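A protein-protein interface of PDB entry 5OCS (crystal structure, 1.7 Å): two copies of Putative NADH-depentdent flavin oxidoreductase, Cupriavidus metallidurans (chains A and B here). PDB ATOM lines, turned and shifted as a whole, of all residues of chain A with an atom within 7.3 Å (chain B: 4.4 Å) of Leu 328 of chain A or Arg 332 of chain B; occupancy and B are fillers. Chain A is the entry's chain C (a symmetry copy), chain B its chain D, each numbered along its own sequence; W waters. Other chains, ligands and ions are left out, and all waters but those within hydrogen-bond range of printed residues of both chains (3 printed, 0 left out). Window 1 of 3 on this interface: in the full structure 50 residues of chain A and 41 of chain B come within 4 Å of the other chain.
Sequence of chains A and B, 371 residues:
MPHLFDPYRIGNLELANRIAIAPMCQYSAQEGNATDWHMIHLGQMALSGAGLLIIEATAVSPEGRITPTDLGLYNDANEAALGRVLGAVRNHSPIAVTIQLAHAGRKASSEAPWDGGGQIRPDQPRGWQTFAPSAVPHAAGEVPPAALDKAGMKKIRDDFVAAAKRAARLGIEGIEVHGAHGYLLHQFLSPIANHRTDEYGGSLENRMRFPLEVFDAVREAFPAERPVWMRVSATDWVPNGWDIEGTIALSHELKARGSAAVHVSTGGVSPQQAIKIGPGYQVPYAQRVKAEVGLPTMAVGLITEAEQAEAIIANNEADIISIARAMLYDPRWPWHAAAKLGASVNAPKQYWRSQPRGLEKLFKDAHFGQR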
ATOM      1  N   ILE A  21      -0.357  31.673   2.777  1.00  0.00           N
ATOM      2  CA  ILE A  21      -1.436  30.967   2.155  1.00  0.00           C
ATOM      3  C   ILE A  21      -2.600  31.964   2.059  1.00  0.00           C
ATOM      4  O   ILE A  21      -3.161  32.416   3.094  1.00  0.00           O
ATOM      5  CB  ILE A  21      -1.808  29.691   2.927  1.00  0.00           C
ATOM      6  CG1 ILE A  21      -0.561  28.833   3.113  1.00  0.00           C
ATOM      7  CG2 ILE A  21      -2.906  28.961   2.197  1.00  0.00           C
ATOM      8  CD1 ILE A  21      -0.752  27.633   4.017  1.00  0.00           C
ATOM      9  N   ALA A  22      -2.916  32.337   0.823  1.00  0.00           N
ATOM     10  CA  ALA A  22      -3.962  33.313   0.571  1.00  0.00           C
ATOM     11  C   ALA A  22      -5.335  32.779   1.010  1.00  0.00           C
ATOM     12  O   ALA A  22      -5.572  31.546   0.975  1.00  0.00           O
ATOM     13  CB  ALA A  22      -3.982  33.640  -0.920  1.00  0.00           C
ATOM     14  N   MET A  24      -8.871  31.365   0.914  1.00  0.00           N
ATOM     15  CA  MET A  24      -9.537  30.542  -0.126  1.00  0.00           C
ATOM     16  C   MET A  24     -10.831  29.951   0.377  1.00  0.00           C
ATOM     17  O   MET A  24     -10.824  28.975   1.096  1.00  0.00           O
ATOM     18  CB  MET A  24      -8.656  29.419  -0.682  1.00  0.00           C
ATOM     19  CG  MET A  24      -7.505  29.907  -1.499  1.00  0.00           C
ATOM     20  SD  MET A  24      -6.419  28.553  -2.057  1.00  0.00           S
ATOM     21  CE  MET A  24      -5.500  28.226  -0.536  1.00  0.00           C
ATOM     22  N   CYS A  25     -11.941  30.561  -0.022  1.00  0.00           N
ATOM     23  CA  CYS A  25     -13.276  30.025   0.252  1.00  0.00           C
ATOM     24  C   CYS A  25     -13.401  28.577  -0.133  1.00  0.00           C
ATOM     25  O   CYS A  25     -13.029  28.177  -1.249  1.00  0.00           O
ATOM     26  CB  CYS A  25     -14.328  30.784  -0.535  1.00  0.00           C
ATOM     27  SG  CYS A  25     -14.736  32.399   0.181  1.00  0.00           S
ATOM     28  N   GLN A  26     -13.940  27.807   0.804  1.00  0.00           N
ATOM     29  CA  GLN A  26     -14.222  26.394   0.615  1.00  0.00           C
ATOM     30  C   GLN A  26     -15.686  26.078   0.399  1.00  0.00           C
ATOM     31  O   GLN A  26     -16.030  24.959   0.003  1.00  0.00           O
ATOM     32  CB  GLN A  26     -13.704  25.630   1.841  1.00  0.00           C
ATOM     33  CG  GLN A  26     -12.227  25.844   2.116  1.00  0.00           C
ATOM     34  CD  GLN A  26     -11.397  25.324   0.935  1.00  0.00           C
ATOM     35  OE1 GLN A  26     -11.425  24.135   0.658  1.00  0.00           O
ATOM     36  NE2 GLN A  26     -10.809  26.224   0.163  1.00  0.00           N
ATOM     37  N   HIS A  41      -8.871  20.471   5.643  1.00  0.00           N
ATOM     38  CA  HIS A  41      -8.284  21.490   4.774  1.00  0.00           C
ATOM     39  C   HIS A  41      -7.320  22.413   5.503  1.00  0.00           C
ATOM     40  O   HIS A  41      -6.148  22.527   5.120  1.00  0.00           O
ATOM     41  CB  HIS A  41      -9.416  22.283   4.136  1.00  0.00           C
ATOM     42  CG  HIS A  41      -8.936  23.459   3.393  1.00  0.00           C
ATOM     43  ND1 HIS A  41      -8.207  23.345   2.234  1.00  0.00           N
ATOM     44  CD2 HIS A  41      -9.080  24.777   3.633  1.00  0.00           C
ATOM     45  CE1 HIS A  41      -7.883  24.562   1.810  1.00  0.00           C
ATOM     46  NE2 HIS A  41      -8.405  25.443   2.643  1.00  0.00           N
ATOM     47  N   GLN A  44      -4.328  20.482   6.913  1.00  0.00           N
ATOM     48  CA  GLN A  44      -3.269  20.239   5.937  1.00  0.00           C
ATOM     49  C   GLN A  44      -2.529  21.521   5.512  1.00  0.00           C
ATOM     50  O   GLN A  44      -1.313  21.510   5.411  1.00  0.00           O
ATOM     51  CB  GLN A  44      -3.777  19.418   4.762  1.00  0.00           C
ATOM     52  CG  GLN A  44      -4.422  20.194   3.665  1.00  0.00           C
ATOM     53  CD  GLN A  44      -4.992  19.258   2.639  1.00  0.00           C
ATOM     54  OE1 GLN A  44      -4.403  19.100   1.542  1.00  0.00           O
ATOM     55  NE2 GLN A  44      -6.117  18.602   2.995  1.00  0.00           N
ATOM     56  N   MET A  45      -3.229  22.637   5.365  1.00  0.00           N
ATOM     57  CA  MET A  45      -2.556  23.878   5.006  1.00  0.00           C
ATOM     58  C   MET A  45      -1.519  24.249   6.080  1.00  0.00           C
ATOM     59  O   MET A  45      -0.462  24.733   5.790  1.00  0.00           O
ATOM     60  CB  MET A  45      -3.538  25.019   4.832  1.00  0.00           C
ATOM     61  CG  MET A  45      -4.531  24.903   3.699  1.00  0.00           C
ATOM     62  SD  MET A  45      -3.744  25.078   2.099  1.00  0.00           S
ATOM     63  CE  MET A  45      -3.550  23.450   1.560  1.00  0.00           C
ATOM     64  N   ILE A 323       0.023  32.784  -1.996  1.00  0.00           N
ATOM     65  CA  ILE A 323      -0.215  31.712  -2.945  1.00  0.00           C
ATOM     66  C   ILE A 323      -1.555  31.055  -2.598  1.00  0.00           C
ATOM     67  O   ILE A 323      -1.804  30.748  -1.436  1.00  0.00           O
ATOM     68  CB  ILE A 323       0.879  30.686  -2.828  1.00  0.00           C
ATOM     69  CG1 ILE A 323       2.229  31.316  -3.156  1.00  0.00           C
ATOM     70  CG2 ILE A 323       0.637  29.522  -3.774  1.00  0.00           C
ATOM     71  CD1 ILE A 323       3.393  30.480  -2.666  1.00  0.00           C
ATOM     72  N   ALA A 324      -2.391  30.843  -3.591  1.00  0.00           N
ATOM     73  CA  ALA A 324      -3.666  30.155  -3.419  1.00  0.00           C
ATOM     74  C   ALA A 324      -3.701  28.851  -4.194  1.00  0.00           C
ATOM     75  O   ALA A 324      -3.463  27.782  -3.663  1.00  0.00           O
ATOM     76  CB  ALA A 324      -4.814  31.086  -3.801  1.00  0.00           C
ATOM     77  N   ARG A 325      -3.964  28.913  -5.478  1.00  0.00           N
ATOM     78  CA  ARG A 325      -4.122  27.677  -6.225  1.00  0.00           C
ATOM     79  C   ARG A 325      -2.914  26.749  -6.154  1.00  0.00           C
ATOM     80  O   ARG A 325      -3.105  25.521  -6.080  1.00  0.00           O
ATOM     81  CB  ARG A 325      -4.459  27.969  -7.669  1.00  0.00           C
ATOM     82  CG  ARG A 325      -5.893  28.449  -7.830  1.00  0.00           C
ATOM     83  CD  ARG A 325      -6.189  29.000  -9.211  1.00  0.00           C
ATOM     84  NE  ARG A 325      -5.523  30.281  -9.392  1.00  0.00           N
ATOM     85  CZ  ARG A 325      -5.690  31.077 -10.446  1.00  0.00           C
ATOM     86  NH1 ARG A 325      -6.499  30.711 -11.428  1.00  0.00           N
ATOM     87  NH2 ARG A 325      -5.062  32.253 -10.506  1.00  0.00           N
ATOM     88  N   ALA A 326      -1.692  27.276  -6.239  1.00  0.00           N
ATOM     89  CA  ALA A 326      -0.509  26.403  -6.112  1.00  0.00           C
ATOM     90  C   ALA A 326      -0.437  25.660  -4.763  1.00  0.00           C
ATOM     91  O   ALA A 326       0.119  24.550  -4.716  1.00  0.00           O
ATOM     92  CB  ALA A 326       0.776  27.125  -6.393  1.00  0.00           C
ATOM     93  N   MET A 327      -0.997  26.238  -3.688  1.00  0.00           N
ATOM     94  CA  MET A 327      -1.144  25.537  -2.427  1.00  0.00           C
ATOM     95  C   MET A 327      -2.169  24.419  -2.429  1.00  0.00           C
ATOM     96  O   MET A 327      -1.985  23.407  -1.775  1.00  0.00           O
ATOM     97  CB  MET A 327      -1.482  26.493  -1.297  1.00  0.00           C
ATOM     98  CG  MET A 327      -0.380  27.371  -0.810  1.00  0.00           C
ATOM     99  SD  MET A 327       0.995  26.488  -0.027  1.00  0.00           S
ATOM    100  CE  MET A 327       0.184  25.525   1.168  1.00  0.00           C
ATOM    101  N   LEU A 328      -3.281  24.617  -3.113  1.00  0.00           N
ATOM    102  CA  LEU A 328      -4.275  23.557  -3.274  1.00  0.00           C
ATOM    103  C   LEU A 328      -3.679  22.434  -4.110  1.00  0.00           C
ATOM    104  O   LEU A 328      -3.877  21.291  -3.791  1.00  0.00           O
ATOM    105  CB  LEU A 328      -5.549  24.107  -3.915  1.00  0.00           C
ATOM    106  CG  LEU A 328      -6.226  25.240  -3.170  1.00  0.00           C
ATOM    107  CD1 LEU A 328      -7.538  25.567  -3.861  1.00  0.00           C
ATOM    108  CD2 LEU A 328      -6.436  24.884  -1.710  1.00  0.00           C
ATOM    109  N   TYR A 329      -2.902  22.763  -5.145  1.00  0.00           N
ATOM    110  CA  TYR A 329      -2.391  21.762  -6.061  1.00  0.00           C
ATOM    111  C   TYR A 329      -1.162  21.076  -5.490  1.00  0.00           C
ATOM    112  O   TYR A 329      -0.829  19.930  -5.877  1.00  0.00           O
ATOM    113  CB  TYR A 329      -2.090  22.427  -7.403  1.00  0.00           C
ATOM    114  CG  TYR A 329      -1.897  21.445  -8.540  1.00  0.00           C
ATOM    115  CD1 TYR A 329      -2.954  20.708  -9.018  1.00  0.00           C
ATOM    116  CD2 TYR A 329      -0.647  21.274  -9.126  1.00  0.00           C
ATOM    117  CE1 TYR A 329      -2.785  19.823 -10.072  1.00  0.00           C
ATOM    118  CE2 TYR A 329      -0.459  20.392 -10.157  1.00  0.00           C
ATOM    119  CZ  TYR A 329      -1.533  19.683 -10.646  1.00  0.00           C
ATOM    120  OH  TYR A 329      -1.339  18.773 -11.691  1.00  0.00           O
ATOM    121  N   ASP A 330      -0.527  21.743  -4.526  1.00  0.00           N
ATOM    122  CA  ASP A 330       0.644  21.213  -3.817  1.00  0.00           C
ATOM    123  C   ASP A 330       0.673  21.808  -2.417  1.00  0.00           C
ATOM    124  O   ASP A 330       1.305  22.811  -2.188  1.00  0.00           O
ATOM    125  CB  ASP A 330       1.932  21.539  -4.570  1.00  0.00           C
ATOM    126  CG  ASP A 330       3.190  21.052  -3.856  1.00  0.00           C
ATOM    127  OD1 ASP A 330       3.116  20.289  -2.888  1.00  0.00           O
ATOM    128  OD2 ASP A 330       4.286  21.491  -4.267  1.00  0.00           O
ATOM    129  N   PRO A 331       0.010  21.154  -1.469  1.00  0.00           N
ATOM    130  CA  PRO A 331      -0.014  21.685  -0.115  1.00  0.00           C
ATOM    131  C   PRO A 331       1.335  21.586   0.584  1.00  0.00           C
ATOM    132  O   PRO A 331       1.476  22.117   1.690  1.00  0.00           O
ATOM    133  CB  PRO A 331      -1.114  20.872   0.574  1.00  0.00           C
ATOM    134  CG  PRO A 331      -1.190  19.602  -0.201  1.00  0.00           C
ATOM    135  CD  PRO A 331      -0.812  19.947  -1.616  1.00  0.00           C
ATOM    136  N   ARG A 332       2.336  20.996  -0.061  1.00  0.00           N
ATOM    137  CA  ARG A 332       3.680  20.987   0.434  1.00  0.00           C
ATOM    138  C   ARG A 332       4.528  22.004  -0.326  1.00  0.00           C
ATOM    139  O   ARG A 332       5.759  21.947  -0.293  1.00  0.00           O
ATOM    140  CB  ARG A 332       4.317  19.597   0.322  1.00  0.00           C
ATOM    141  CG  ARG A 332       3.468  18.443   0.831  1.00  0.00           C
ATOM    142  CD  ARG A 332       3.258  18.432   2.334  1.00  0.00           C
ATOM    143  NE  ARG A 332       2.789  17.110   2.731  1.00  0.00           N
ATOM    144  CZ  ARG A 332       1.592  16.793   3.228  1.00  0.00           C
ATOM    145  NH1 ARG A 332       0.679  17.720   3.535  1.00  0.00           N
ATOM    146  NH2 ARG A 332       1.319  15.530   3.476  1.00  0.00           N
ATOM    147  N   TRP A 333       3.885  22.950  -1.001  1.00  0.00           N
ATOM    148  CA  TRP A 333       4.616  23.946  -1.822  1.00  0.00           C
ATOM    149  C   TRP A 333       5.806  24.572  -1.100  1.00  0.00           C
ATOM    150  O   TRP A 333       6.887  24.684  -1.687  1.00  0.00           O
ATOM    151  CB  TRP A 333       3.665  25.014  -2.344  1.00  0.00           C
ATOM    152  CG  TRP A 333       4.243  25.866  -3.442  1.00  0.00           C
ATOM    153  CD1 TRP A 333       4.083  25.689  -4.793  1.00  0.00           C
ATOM    154  CD2 TRP A 333       5.057  27.025  -3.272  1.00  0.00           C
ATOM    155  NE1 TRP A 333       4.783  26.681  -5.480  1.00  0.00           N
ATOM    156  CE2 TRP A 333       5.373  27.515  -4.555  1.00  0.00           C
ATOM    157  CE3 TRP A 333       5.558  27.711  -2.142  1.00  0.00           C
ATOM    158  CZ2 TRP A 333       6.174  28.630  -4.745  1.00  0.00           C
ATOM    159  CZ3 TRP A 333       6.341  28.817  -2.345  1.00  0.00           C
ATOM    160  CH2 TRP A 333       6.644  29.272  -3.627  1.00  0.00           C
ATOM    161  N   ASP B 330       4.165  14.391  -1.167  1.00  0.00           N
ATOM    162  CA  ASP B 330       3.201  14.939  -2.194  1.00  0.00           C
ATOM    163  C   ASP B 330       1.846  14.220  -2.067  1.00  0.00           C
ATOM    164  O   ASP B 330       1.559  13.222  -2.757  1.00  0.00           O
ATOM    165  CB  ASP B 330       3.755  14.768  -3.607  1.00  0.00           C
ATOM    166  CG  ASP B 330       2.839  15.318  -4.690  1.00  0.00           C
ATOM    167  OD1 ASP B 330       1.778  15.952  -4.389  1.00  0.00           O
ATOM    168  OD2 ASP B 330       3.173  15.050  -5.885  1.00  0.00           O
ATOM    169  N   PRO B 331       0.960  14.704  -1.181  1.00  0.00           N
ATOM    170  CA  PRO B 331      -0.332  14.054  -1.030  1.00  0.00           C
ATOM    171  C   PRO B 331      -1.239  14.206  -2.221  1.00  0.00           C
ATOM    172  O   PRO B 331      -2.270  13.571  -2.256  1.00  0.00           O
ATOM    173  CB  PRO B 331      -0.952  14.775   0.183  1.00  0.00           C
ATOM    174  CG  PRO B 331      -0.300  16.083   0.143  1.00  0.00           C
ATOM    175  CD  PRO B 331       1.108  15.825  -0.260  1.00  0.00           C
ATOM    176  N   ARG B 332      -0.848  15.033  -3.199  1.00  0.00           N
ATOM    177  CA  ARG B 332      -1.514  15.094  -4.476  1.00  0.00           C
ATOM    178  C   ARG B 332      -0.802  14.254  -5.559  1.00  0.00           C
ATOM    179  O   ARG B 332      -1.051  14.451  -6.783  1.00  0.00           O
ATOM    180  CB  ARG B 332      -1.617  16.547  -4.951  1.00  0.00           C
ATOM    181  CG  ARG B 332      -2.225  17.505  -3.924  1.00  0.00           C
ATOM    182  CD  ARG B 332      -3.679  17.214  -3.591  1.00  0.00           C
ATOM    183  NE  ARG B 332      -4.162  18.418  -2.923  1.00  0.00           N
ATOM    184  CZ  ARG B 332      -4.389  18.590  -1.629  1.00  0.00           C
ATOM    185  NH1 ARG B 332      -4.427  17.584  -0.782  1.00  0.00           N
ATOM    186  NH2 ARG B 332      -4.677  19.821  -1.206  1.00  0.00           N
ATOM    187  N   TRP B 333       0.069  13.330  -5.150  1.00  0.00           N
ATOM    188  CA  TRP B 333       0.814  12.508  -6.104  1.00  0.00           C
ATOM    189  C   TRP B 333      -0.042  11.923  -7.240  1.00  0.00           C
ATOM    190  O   TRP B 333       0.366  12.012  -8.433  1.00  0.00           O
ATOM    191  CB  TRP B 333       1.589  11.384  -5.381  1.00  0.00           C
ATOM    192  CG  TRP B 333       2.612  10.683  -6.269  1.00  0.00           C
ATOM    193  CD1 TRP B 333       3.919  10.986  -6.366  1.00  0.00           C
ATOM    194  CD2 TRP B 333       2.377   9.594  -7.183  1.00  0.00           C
ATOM    195  NE1 TRP B 333       4.538  10.170  -7.280  1.00  0.00           N
ATOM    196  CE2 TRP B 333       3.622   9.296  -7.789  1.00  0.00           C
ATOM    197  CE3 TRP B 333       1.250   8.826  -7.519  1.00  0.00           C
ATOM    198  CZ2 TRP B 333       3.776   8.280  -8.727  1.00  0.00           C
ATOM    199  CZ3 TRP B 333       1.399   7.800  -8.474  1.00  0.00           C
ATOM    200  CH2 TRP B 333       2.669   7.554  -9.061  1.00  0.00           C
ATOM    201  N   PRO B 334      -1.239  11.397  -6.938  1.00  0.00           N
ATOM    202  CA  PRO B 334      -2.018  10.837  -8.046  1.00  0.00           C
ATOM    203  C   PRO B 334      -2.506  11.919  -9.000  1.00  0.00           C
ATOM    204  O   PRO B 334      -2.562  11.679 -10.221  1.00  0.00           O
ATOM    205  CB  PRO B 334      -3.181  10.097  -7.364  1.00  0.00           C
ATOM    206  CG  PRO B 334      -2.715   9.905  -5.911  1.00  0.00           C
ATOM    207  CD  PRO B 334      -1.871  11.109  -5.627  1.00  0.00           C
ATOM    208  N   TRP B 335      -2.807  13.126  -8.505  1.00  0.00           N
ATOM    209  CA  TRP B 335      -3.128  14.217  -9.461  1.00  0.00           C
ATOM    210  C   TRP B 335      -1.933  14.534 -10.421  1.00  0.00           C
ATOM    211  O   TRP B 335      -2.074  14.687 -11.661  1.00  0.00           O
ATOM    212  CB  TRP B 335      -3.438  15.505  -8.745  1.00  0.00           C
ATOM    213  CG  TRP B 335      -4.580  15.506  -7.782  1.00  0.00           C
ATOM    214  CD1 TRP B 335      -5.310  14.451  -7.322  1.00  0.00           C
ATOM    215  CD2 TRP B 335      -5.060  16.668  -7.099  1.00  0.00           C
ATOM    216  NE1 TRP B 335      -6.264  14.901  -6.426  1.00  0.00           N
ATOM    217  CE2 TRP B 335      -6.134  16.264  -6.294  1.00  0.00           C
ATOM    218  CE3 TRP B 335      -4.709  18.027  -7.147  1.00  0.00           C
ATOM    219  CZ2 TRP B 335      -6.834  17.176  -5.481  1.00  0.00           C
ATOM    220  CZ3 TRP B 335      -5.396  18.914  -6.355  1.00  0.00           C
ATOM    221  CH2 TRP B 335      -6.451  18.480  -5.535  1.00  0.00           C
ATOM    222  N   HIS B 336      -0.755  14.615  -9.824  1.00  0.00           N
ATOM    223  CA  HIS B 336       0.479  14.956 -10.537  1.00  0.00           C
ATOM    224  C   HIS B 336       0.848  13.861 -11.508  1.00  0.00           C
ATOM    225  O   HIS B 336       1.237  14.190 -12.661  1.00  0.00           O
ATOM    226  CB  HIS B 336       1.572  15.298  -9.570  1.00  0.00           C
ATOM    227  CG  HIS B 336       1.215  16.448  -8.702  1.00  0.00           C
ATOM    228  ND1 HIS B 336       1.720  16.614  -7.432  1.00  0.00           N
ATOM    229  CD2 HIS B 336       0.308  17.434  -8.885  1.00  0.00           C
ATOM    230  CE1 HIS B 336       1.200  17.709  -6.897  1.00  0.00           C
ATOM    231  NE2 HIS B 336       0.345  18.233  -7.771  1.00  0.00           N
ATOM    232  N   TYR B 351     -11.490  21.891  -4.547  1.00  0.00           N
ATOM    233  CA  TYR B 351     -10.170  22.092  -5.103  1.00  0.00           C
ATOM    234  C   TYR B 351     -10.131  22.069  -6.624  1.00  0.00           C
ATOM    235  O   TYR B 351      -9.052  22.155  -7.217  1.00  0.00           O
ATOM    236  CB  TYR B 351      -9.237  21.008  -4.573  1.00  0.00           C
ATOM    237  CG  TYR B 351      -8.931  21.018  -3.108  1.00  0.00           C
ATOM    238  CD1 TYR B 351      -9.208  22.108  -2.297  1.00  0.00           C
ATOM    239  CD2 TYR B 351      -8.355  19.892  -2.526  1.00  0.00           C
ATOM    240  CE1 TYR B 351      -8.879  22.108  -0.957  1.00  0.00           C
ATOM    241  CE2 TYR B 351      -8.035  19.849  -1.178  1.00  0.00           C
ATOM    242  CZ  TYR B 351      -8.282  20.974  -0.397  1.00  0.00           C
ATOM    243  OH  TYR B 351      -7.946  20.929   0.941  1.00  0.00           O
ATOM    244  N   SER B 354      -7.869  24.501  -8.602  1.00  0.00           N
ATOM    245  CA  SER B 354      -6.423  24.382  -8.466  1.00  0.00           C
ATOM    246  C   SER B 354      -5.668  23.933  -9.696  1.00  0.00           C
ATOM    247  O   SER B 354      -4.441  23.976  -9.682  1.00  0.00           O
ATOM    248  CB  SER B 354      -6.090  23.393  -7.344  1.00  0.00           C
ATOM    249  OG  SER B 354      -6.349  22.070  -7.693  1.00  0.00           O
HETATM  250  O   HOH W   1      -7.168  16.884   0.819  1.00  0.00           O
HETATM  251  O   HOH W   2       1.493  17.997  -2.603  1.00  0.00           O
HETATM  252  O   HOH W   3      -9.124  18.769   2.038  1.00  0.00           O
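Water W3 lies within hydrogen-bond range of OH of Tyr 351 of chain B (2.7 Å) and NE2 of Gln 44 of chain A (3.2 Å).
Water W2 lies within hydrogen-bond range of OD1 of Asp 330 of chain B and OD1 of Asp 330 of chain A.
Water W1 lies within hydrogen-bond range of NE2 of Gln 44 of chain A (3.0 Å) and NH1 of Arg 332 of chain B (3.3 Å).
Of the printed residues of chain B, Gln 26 of chain A touches Tyr 351 (3.6 Å).
Of the printed residues of chain B, His 41 of chain A touches Tyr 351 (2.8 Å).
Ala 326 of chain A touches none of the printed residues of chain B.
Leu 328 of chain A touches four residues of chain B.
Printed residues of chain B within 4 Å of Pro 331 of chain A: Pro 331 (3.6 Å) and Arg 332 (3.6 Å).
Of chain A, only Gln 44, Leu 328, Tyr 329 and Pro 331 come within 4 Å of Arg 332 of chain B.
Of the printed residues of chain A, His 336 of chain B touches Tyr 329 (2.8 Å).
The nearest residue of chain A that does not touch Arg 332 of chain B is Met 327 of chain A (4.5 Å).
Gln 26 of chain A touches Tyr 351 of chain B.
Tyr 351 of chain B touches Gln 44 of chain A (OH to NE2, 3.6 Å).
Trp 335 of chain B touches Leu 328 of chain A.
CE1 of Tyr 351 of chain B touches CD2 of Leu 328 of chain A, 3.8 Å away.
Tyr 329 of chain A touches Arg 332 of chain B.
Tyr 329 of chain A touches Trp 335 of chain B (CD1 to CE3, 3.7 Å).
CB of Tyr 329 of chain A touches O of Ser 354 of chain B (3.6 Å).
Pro 331 of chain A touches Pro 331 of chain B.
Pro 331 of chain A touches Arg 332 of chain B (CG to NH2, 3.6 Å).
CD of Pro 331 of chain B touches CZ of Arg 332 of chain A, at 3.7 Å.
O of Leu 328 of chain A lies within hydrogen-bond range of NE of Arg 332 of chain B (3.0 Å).
NH1 of Arg 332 of chain B lies within hydrogen-bond range of OE1 of Gln 44 of chain A (2.8 Å).
The side-chain hydroxyl (OH) of Tyr 351 of chain B is in hydrogen-bond range of a ring nitrogen (ND1) of His 41 of chain A (2.8 Å).
NE2 of His 336 of chain B lies within hydrogen-bond range of O of Tyr 329 of chain A (2.8 Å).
The side-chain hydroxyl of Ser 354 of chain B sits at hydrogen-bond distance from the backbone carbonyl oxygen of Tyr 351 of chain B (2.7 Å).
ND1 of His 336 of chain B lies within hydrogen-bond range of OD2 of Asp 330 of chain B, 2.6 Å away.
O of Met 24 of chain A sits at hydrogen-bond distance from NE2 of Gln 26 of chain A, 2.9 Å away.
OD1 of Asp 330 of chain A lies close to N of Arg 332 of chain A (3.0 Å).
OD1 of Asp 330 of chain B lies within hydrogen-bond range of N of Arg 332 of chain B (3.0 Å).
Pro 331 of chain B touches its own counterpart, Pro 331 of chain A.
Pro 331 of chain A touches Arg 332 of chain B, and with the chains exchanged Arg 332 of chain A touches Pro 331 of chain B.
Positions printed for both chains: 330, 331, 332 and 333.
Of the 16 pairs that touch across the chains among the printed residues, 3 have their exchanged pair printed and touching as well.
Printed residues of chain B that touch a printed residue of chain A: Pro 331, Arg 332, Trp 335, His 336, Tyr 351 and Ser 354.
Hydrophobic or aromatic side chains of chain B within 4 Å of the printed part of chain A: Pro 331, Trp 335, His 336 and Tyr 351.
Among the printed residues, 16 pairs touch across the chains.
Among the printed residues, no Asp or Glu carboxylate lies within 4 Å of a Lys or Arg side-chain nitrogen of the other chain.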
